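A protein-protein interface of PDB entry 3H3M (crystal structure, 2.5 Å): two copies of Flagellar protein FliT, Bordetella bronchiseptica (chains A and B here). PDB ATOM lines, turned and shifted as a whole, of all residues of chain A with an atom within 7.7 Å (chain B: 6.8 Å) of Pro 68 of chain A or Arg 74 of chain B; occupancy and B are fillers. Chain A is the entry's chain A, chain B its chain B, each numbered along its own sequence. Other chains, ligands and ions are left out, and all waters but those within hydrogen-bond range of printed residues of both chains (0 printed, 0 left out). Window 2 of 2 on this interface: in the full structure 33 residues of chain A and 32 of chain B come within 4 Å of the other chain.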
ATOM      1  N   ALA A  18     -33.063 -17.663 -25.778  1.00  0.00           N
ATOM      2  CA  ALA A  18     -32.291 -17.220 -26.994  1.00  0.00           C
ATOM      3  C   ALA A  18     -31.030 -18.123 -27.190  1.00  0.00           C
ATOM      4  O   ALA A  18     -30.593 -18.838 -26.230  1.00  0.00           O
ATOM      5  CB  ALA A  18     -31.902 -15.719 -26.881  1.00  0.00           C
ATOM      6  N   GLU A  64     -22.579 -12.581 -31.649  1.00  0.00           N
ATOM      7  CA  GLU A  64     -22.476 -11.406 -30.808  1.00  0.00           C
ATOM      8  C   GLU A  64     -21.665 -10.293 -31.474  1.00  0.00           C
ATOM      9  O   GLU A  64     -20.730 -10.576 -32.233  1.00  0.00           O
ATOM     10  CB  GLU A  64     -21.841 -11.788 -29.462  1.00  0.00           C
ATOM     11  CG  GLU A  64     -22.787 -12.472 -28.492  1.00  0.00           C
ATOM     12  CD  GLU A  64     -23.502 -11.497 -27.560  1.00  0.00           C
ATOM     13  OE1 GLU A  64     -24.008 -10.460 -28.033  1.00  0.00           O
ATOM     14  OE2 GLU A  64     -23.559 -11.771 -26.344  1.00  0.00           O
ATOM     15  N   PRO A  65     -21.999  -9.017 -31.160  1.00  0.00           N
ATOM     16  CA  PRO A  65     -23.096  -8.655 -30.230  1.00  0.00           C
ATOM     17  C   PRO A  65     -24.508  -8.509 -30.836  1.00  0.00           C
ATOM     18  O   PRO A  65     -24.751  -8.782 -32.057  1.00  0.00           O
ATOM     19  CB  PRO A  65     -22.650  -7.296 -29.635  1.00  0.00           C
ATOM     20  CG  PRO A  65     -21.434  -6.885 -30.369  1.00  0.00           C
ATOM     21  CD  PRO A  65     -21.276  -7.807 -31.588  1.00  0.00           C
ATOM     22  N   GLY A  66     -25.412  -8.100 -29.937  1.00  0.00           N
ATOM     23  CA  GLY A  66     -26.814  -7.854 -30.257  1.00  0.00           C
ATOM     24  C   GLY A  66     -27.616  -9.148 -30.278  1.00  0.00           C
ATOM     25  O   GLY A  66     -27.093 -10.238 -29.898  1.00  0.00           O
ATOM     26  N   GLU A  67     -28.915  -9.029 -30.610  1.00  0.00           N
ATOM     27  CA  GLU A  67     -29.664  -7.762 -30.467  1.00  0.00           C
ATOM     28  C   GLU A  67     -29.700  -7.614 -28.930  1.00  0.00           C
ATOM     29  O   GLU A  67     -29.041  -8.453 -28.248  1.00  0.00           O
ATOM     30  CB  GLU A  67     -31.066  -7.925 -31.107  1.00  0.00           C
ATOM     31  CG  GLU A  67     -31.074  -8.321 -32.646  1.00  0.00           C
ATOM     32  CD  GLU A  67     -31.360  -7.115 -33.629  1.00  0.00           C
ATOM     33  OE1 GLU A  67     -31.008  -5.915 -33.313  1.00  0.00           O
ATOM     34  OE2 GLU A  67     -31.950  -7.383 -34.732  1.00  0.00           O
ATOM     35  N   PRO A  68     -30.426  -6.587 -28.354  1.00  0.00           N
ATOM     36  CA  PRO A  68     -30.379  -6.454 -26.862  1.00  0.00           C
ATOM     37  C   PRO A  68     -30.814  -7.766 -26.214  1.00  0.00           C
ATOM     38  O   PRO A  68     -31.108  -8.711 -26.970  1.00  0.00           O
ATOM     39  CB  PRO A  68     -31.394  -5.316 -26.541  1.00  0.00           C
ATOM     40  CG  PRO A  68     -31.829  -4.707 -27.898  1.00  0.00           C
ATOM     41  CD  PRO A  68     -31.566  -5.828 -28.921  1.00  0.00           C
ATOM     42  N   LEU A  69     -30.855  -7.839 -24.876  1.00  0.00           N
ATOM     43  CA  LEU A  69     -31.282  -9.061 -24.160  1.00  0.00           C
ATOM     44  C   LEU A  69     -32.369  -8.767 -23.097  1.00  0.00           C
ATOM     45  O   LEU A  69     -32.510  -7.634 -22.647  1.00  0.00           O
ATOM     46  CB  LEU A  69     -30.072  -9.799 -23.546  1.00  0.00           C
ATOM     47  CG  LEU A  69     -29.433 -10.915 -24.383  1.00  0.00           C
ATOM     48  N   ASP A  70     -33.072  -9.829 -22.678  1.00  0.00           N
ATOM     49  CA  ASP A  70     -34.402  -9.778 -22.028  1.00  0.00           C
ATOM     50  C   ASP A  70     -34.574  -9.382 -20.533  1.00  0.00           C
ATOM     51  O   ASP A  70     -35.687  -9.504 -20.002  1.00  0.00           O
ATOM     52  CB  ASP A  70     -35.087 -11.144 -22.236  1.00  0.00           C
ATOM     53  N   GLU A  71     -33.515  -8.912 -19.865  1.00  0.00           N
ATOM     54  CA  GLU A  71     -33.501  -8.659 -18.394  1.00  0.00           C
ATOM     55  C   GLU A  71     -33.401  -9.952 -17.588  1.00  0.00           C
ATOM     56  O   GLU A  71     -32.553 -10.067 -16.696  1.00  0.00           O
ATOM     57  CB  GLU A  71     -34.693  -7.827 -17.902  1.00  0.00           C
ATOM     58  CG  GLU A  71     -34.571  -7.354 -16.446  1.00  0.00           C
ATOM     59  N   ALA A  73     -32.773 -12.833 -19.282  1.00  0.00           N
ATOM     60  CA  ALA A  73     -31.616 -13.390 -19.980  1.00  0.00           C
ATOM     61  C   ALA A  73     -30.329 -12.546 -19.838  1.00  0.00           C
ATOM     62  O   ALA A  73     -29.280 -12.977 -20.282  1.00  0.00           O
ATOM     63  CB  ALA A  73     -31.952 -13.613 -21.454  1.00  0.00           C
ATOM     64  N   ARG A  74     -30.411 -11.357 -19.235  1.00  0.00           N
ATOM     65  CA  ARG A  74     -29.235 -10.505 -18.974  1.00  0.00           C
ATOM     66  C   ARG A  74     -28.515 -11.002 -17.720  1.00  0.00           C
ATOM     67  O   ARG A  74     -27.308 -11.279 -17.745  1.00  0.00           O
ATOM     68  CB  ARG A  74     -29.650  -9.031 -18.799  1.00  0.00           C
ATOM     69  CG  ARG A  74     -28.702  -8.019 -19.470  1.00  0.00           C
ATOM     70  CD  ARG A  74     -29.112  -6.566 -19.217  1.00  0.00           C
ATOM     71  NE  ARG A  74     -30.383  -6.231 -19.873  1.00  0.00           N
ATOM     72  CZ  ARG A  74     -31.560  -6.033 -19.262  1.00  0.00           C
ATOM     73  NH1 ARG A  74     -31.688  -6.131 -17.935  1.00  0.00           N
ATOM     74  NH2 ARG A  74     -32.634  -5.724 -19.991  1.00  0.00           N
ATOM     75  N   LYS A  77     -26.719 -14.371 -18.302  1.00  0.00           N
ATOM     76  CA  LYS A  77     -25.457 -14.292 -19.042  1.00  0.00           C
ATOM     77  C   LYS A  77     -24.421 -13.755 -18.080  1.00  0.00           C
ATOM     78  O   LYS A  77     -23.373 -14.341 -17.925  1.00  0.00           O
ATOM     79  CB  LYS A  77     -25.604 -13.424 -20.305  1.00  0.00           C
ATOM     80  CG  LYS A  77     -24.324 -12.902 -20.930  1.00  0.00           C
ATOM     81  CD  LYS A  77     -24.649 -12.078 -22.206  1.00  0.00           C
ATOM     82  CE  LYS A  77     -23.673 -10.921 -22.462  1.00  0.00           C
ATOM     83  NZ  LYS A  77     -24.286  -9.595 -22.124  1.00  0.00           N
ATOM     84  N   LEU B  21     -18.607  -1.394 -17.580  1.00  0.00           N
ATOM     85  CA  LEU B  21     -17.537  -1.384 -18.596  1.00  0.00           C
ATOM     86  C   LEU B  21     -16.178  -1.129 -17.957  1.00  0.00           C
ATOM     87  O   LEU B  21     -15.172  -1.677 -18.423  1.00  0.00           O
ATOM     88  CB  LEU B  21     -17.775  -0.328 -19.705  1.00  0.00           C
ATOM     89  CG  LEU B  21     -19.096  -0.371 -20.486  1.00  0.00           C
ATOM     90  CD1 LEU B  21     -19.201   0.779 -21.525  1.00  0.00           C
ATOM     91  CD2 LEU B  21     -19.306  -1.726 -21.162  1.00  0.00           C
ATOM     92  N   LEU B  69     -28.122  -1.085 -21.156  1.00  0.00           N
ATOM     93  CA  LEU B  69     -26.896  -1.039 -21.986  1.00  0.00           C
ATOM     94  C   LEU B  69     -27.188  -0.799 -23.494  1.00  0.00           C
ATOM     95  O   LEU B  69     -27.765  -1.667 -24.166  1.00  0.00           O
ATOM     96  CB  LEU B  69     -26.065  -2.326 -21.802  1.00  0.00           C
ATOM     97  N   ASP B  70     -26.785   0.369 -24.021  1.00  0.00           N
ATOM     98  CA  ASP B  70     -27.017   0.710 -25.446  1.00  0.00           C
ATOM     99  C   ASP B  70     -26.076  -0.092 -26.375  1.00  0.00           C
ATOM    100  O   ASP B  70     -25.179  -0.797 -25.887  1.00  0.00           O
ATOM    101  CB  ASP B  70     -26.961   2.232 -25.694  1.00  0.00           C
ATOM    102  CG  ASP B  70     -25.557   2.769 -25.848  1.00  0.00           C
ATOM    103  OD1 ASP B  70     -25.408   4.006 -25.973  1.00  0.00           O
ATOM    104  OD2 ASP B  70     -24.603   1.978 -25.866  1.00  0.00           O
ATOM    105  N   GLU B  71     -26.285  -0.001 -27.693  1.00  0.00           N
ATOM    106  CA  GLU B  71     -25.691  -0.975 -28.636  1.00  0.00           C
ATOM    107  C   GLU B  71     -24.167  -0.800 -28.744  1.00  0.00           C
ATOM    108  O   GLU B  71     -23.413  -1.804 -28.707  1.00  0.00           O
ATOM    109  CB  GLU B  71     -26.394  -0.926 -30.020  1.00  0.00           C
ATOM    110  CG  GLU B  71     -25.935  -2.045 -31.021  1.00  0.00           C
ATOM    111  CD  GLU B  71     -27.087  -2.725 -31.805  1.00  0.00           C
ATOM    112  OE1 GLU B  71     -27.681  -2.055 -32.684  1.00  0.00           O
ATOM    113  OE2 GLU B  71     -27.370  -3.937 -31.550  1.00  0.00           O
ATOM    114  N   ALA B  72     -23.740   0.470 -28.867  1.00  0.00           N
ATOM    115  CA  ALA B  72     -22.331   0.869 -28.806  1.00  0.00           C
ATOM    116  C   ALA B  72     -21.676   0.317 -27.550  1.00  0.00           C
ATOM    117  O   ALA B  72     -20.546  -0.162 -27.590  1.00  0.00           O
ATOM    118  CB  ALA B  72     -22.208   2.388 -28.812  1.00  0.00           C
ATOM    119  N   ALA B  73     -22.401   0.378 -26.437  1.00  0.00           N
ATOM    120  CA  ALA B  73     -21.905  -0.094 -25.153  1.00  0.00           C
ATOM    121  C   ALA B  73     -21.828  -1.618 -25.116  1.00  0.00           C
ATOM    122  O   ALA B  73     -20.954  -2.164 -24.485  1.00  0.00           O
ATOM    123  CB  ALA B  73     -22.784   0.424 -24.028  1.00  0.00           C
ATOM    124  N   ARG B  74     -22.746  -2.302 -25.788  1.00  0.00           N
ATOM    125  CA  ARG B  74     -22.728  -3.756 -25.785  1.00  0.00           C
ATOM    126  C   ARG B  74     -21.644  -4.264 -26.732  1.00  0.00           C
ATOM    127  O   ARG B  74     -21.023  -5.274 -26.447  1.00  0.00           O
ATOM    128  CB  ARG B  74     -24.112  -4.368 -26.101  1.00  0.00           C
ATOM    129  CG  ARG B  74     -25.242  -3.932 -25.133  1.00  0.00           C
ATOM    130  CD  ARG B  74     -26.473  -4.916 -25.077  1.00  0.00           C
ATOM    131  NE  ARG B  74     -26.915  -5.346 -26.407  1.00  0.00           N
ATOM    132  CZ  ARG B  74     -27.540  -4.570 -27.294  1.00  0.00           C
ATOM    133  NH1 ARG B  74     -27.831  -3.296 -27.016  1.00  0.00           N
ATOM    134  NH2 ARG B  74     -27.890  -5.076 -28.475  1.00  0.00           N
ATOM    135  N   GLY B  75     -21.397  -3.557 -27.827  1.00  0.00           N
ATOM    136  CA  GLY B  75     -20.251  -3.868 -28.675  1.00  0.00           C
ATOM    137  C   GLY B  75     -18.941  -3.707 -27.925  1.00  0.00           C
ATOM    138  O   GLY B  75     -18.020  -4.495 -28.061  1.00  0.00           O
ATOM    139  N   MET B  76     -18.873  -2.676 -27.109  1.00  0.00           N
ATOM    140  CA  MET B  76     -17.689  -2.403 -26.297  1.00  0.00           C
ATOM    141  C   MET B  76     -17.412  -3.499 -25.278  1.00  0.00           C
ATOM    142  O   MET B  76     -16.287  -3.980 -25.175  1.00  0.00           O
ATOM    143  CB  MET B  76     -17.927  -1.105 -25.547  1.00  0.00           C
ATOM    144  CG  MET B  76     -16.699  -0.318 -25.140  1.00  0.00           C
ATOM    145  SD  MET B  76     -17.080   1.599 -25.550  1.00  0.00           S
ATOM    146  CE  MET B  76     -19.059   1.804 -25.305  1.00  0.00           C
ATOM    147  N   LYS B  77     -18.444  -3.853 -24.508  1.00  0.00           N
ATOM    148  CA  LYS B  77     -18.378  -4.931 -23.530  1.00  0.00           C
ATOM    149  C   LYS B  77     -17.999  -6.241 -24.198  1.00  0.00           C
ATOM    150  O   LYS B  77     -17.116  -6.954 -23.701  1.00  0.00           O
ATOM    151  CB  LYS B  77     -19.733  -5.148 -22.837  1.00  0.00           C
ATOM    152  CG  LYS B  77     -19.688  -6.195 -21.692  1.00  0.00           C
ATOM    153  CD  LYS B  77     -21.083  -6.678 -21.221  1.00  0.00           C
ATOM    154  CE  LYS B  77     -21.440  -8.087 -21.747  1.00  0.00           C
ATOM    155  NZ  LYS B  77     -21.935  -8.980 -20.631  1.00  0.00           N
ATOM    156  N   PHE B  78     -18.693  -6.576 -25.292  1.00  0.00           N
ATOM    157  CA  PHE B  78     -18.436  -7.833 -25.967  1.00  0.00           C
ATOM    158  C   PHE B  78     -16.971  -7.958 -26.438  1.00  0.00           C
ATOM    159  O   PHE B  78     -16.361  -8.980 -26.216  1.00  0.00           O
ATOM    160  CB  PHE B  78     -19.339  -8.072 -27.162  1.00  0.00           C
ATOM    161  CG  PHE B  78     -19.040  -9.349 -27.807  1.00  0.00           C
ATOM    162  CD1 PHE B  78     -19.305 -10.540 -27.120  1.00  0.00           C
ATOM    163  CD2 PHE B  78     -18.353  -9.403 -29.011  1.00  0.00           C
ATOM    164  CE1 PHE B  78     -18.952 -11.780 -27.675  1.00  0.00           C
ATOM    165  CE2 PHE B  78     -18.004 -10.612 -29.570  1.00  0.00           C
ATOM    166  CZ  PHE B  78     -18.305 -11.806 -28.919  1.00  0.00           C
ATOM    167  N   ASP B  79     -16.439  -6.891 -27.042  1.00  0.00           N
ATOM    168  CA  ASP B  79     -15.018  -6.769 -27.403  1.00  0.00           C
ATOM    169  C   ASP B  79     -14.046  -7.006 -26.266  1.00  0.00           C
ATOM    170  O   ASP B  79     -12.955  -7.523 -26.508  1.00  0.00           O
ATOM    171  CB  ASP B  79     -14.689  -5.398 -27.998  1.00  0.00           C
ATOM    172  CG  ASP B  79     -15.297  -5.206 -29.350  1.00  0.00           C
ATOM    173  OD1 ASP B  79     -15.670  -6.215 -29.975  1.00  0.00           O
ATOM    174  OD2 ASP B  79     -15.400  -4.045 -29.806  1.00  0.00           O
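NH2 of Arg 74 of chain B sits close to N of Pro 68 of chain A.
NZ of Lys 77 of chain A lies close to NZ of Lys 77 of chain B.
Of the 12 printed residues of chain A, 6 touch a printed residue of chain B.
Hydrophobic or aromatic side chains of chain A within 4 Å of the printed part of chain B: Pro 65 and Pro 68.
Of the 12 printed residues of chain B, 4 touch a printed residue of chain A.
Printed residues of chain B that touch a printed residue of chain A: Arg 74, Gly 75, Lys 77 and Phe 78.
Hydrophobic or aromatic side chains of chain B that line the printed part of chain A: Phe 78.
Among the printed residues, 6 pairs touch across the chains.
Among the printed residues, no Asp or Glu carboxylate lies within 4 Å of a Lys or Arg side-chain nitrogen of the other chain.
Glu 64 of chain A touches Phe 78 of chain B.
CG of Pro 65 of chain A touches CA of Gly 75 of chain B, 3.7 Å away.
Arg 74 of chain B touches Gly 66 of chain A (NH2 to CA, 3.5 Å).
Glu 67 of chain A touches Arg 74 of chain B.
Lys 77 of chain B touches its own counterpart, Lys 77 of chain A.
Of the printed residues of chain B, Glu 64 of chain A touches Phe 78 (3.4 Å).
Printed residues of chain B within 4 Å of Pro 65 of chain A: Gly 75.
Printed residues of chain B within 4 Å of Glu 67 of chain A: Arg 74 (3.2 Å).
Pro 68 of chain A touches just one residue of chain B: Arg 74.
Ala 72 of chain B touches none of the printed residues of chain A.
Arg 74 of chain B touches just these residues of chain A: Gly 66 (3.5 Å), Glu 67 (3.2 Å) and Pro 68 (3.0 Å).
Gly 75 of chain B touches just one residue of chain A: Pro 65.
Printed residues of chain A within 4 Å of Lys 77 of chain B: Lys 77.
The side-chain carboxylate of Glu 64 of chain A lies within hydrogen-bond range of the backbone NH of Gly 66 of chain A, 3.3 Å away.
O of Leu 69 of chain B sits at hydrogen-bond distance from NH1 of Arg 74 of chain B (3.3 Å).
The side-chain carboxylate of Glu 71 of chain B lies within salt-bridge range of the guanidinium group of Arg 74 of chain B, at 3.3 Å.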
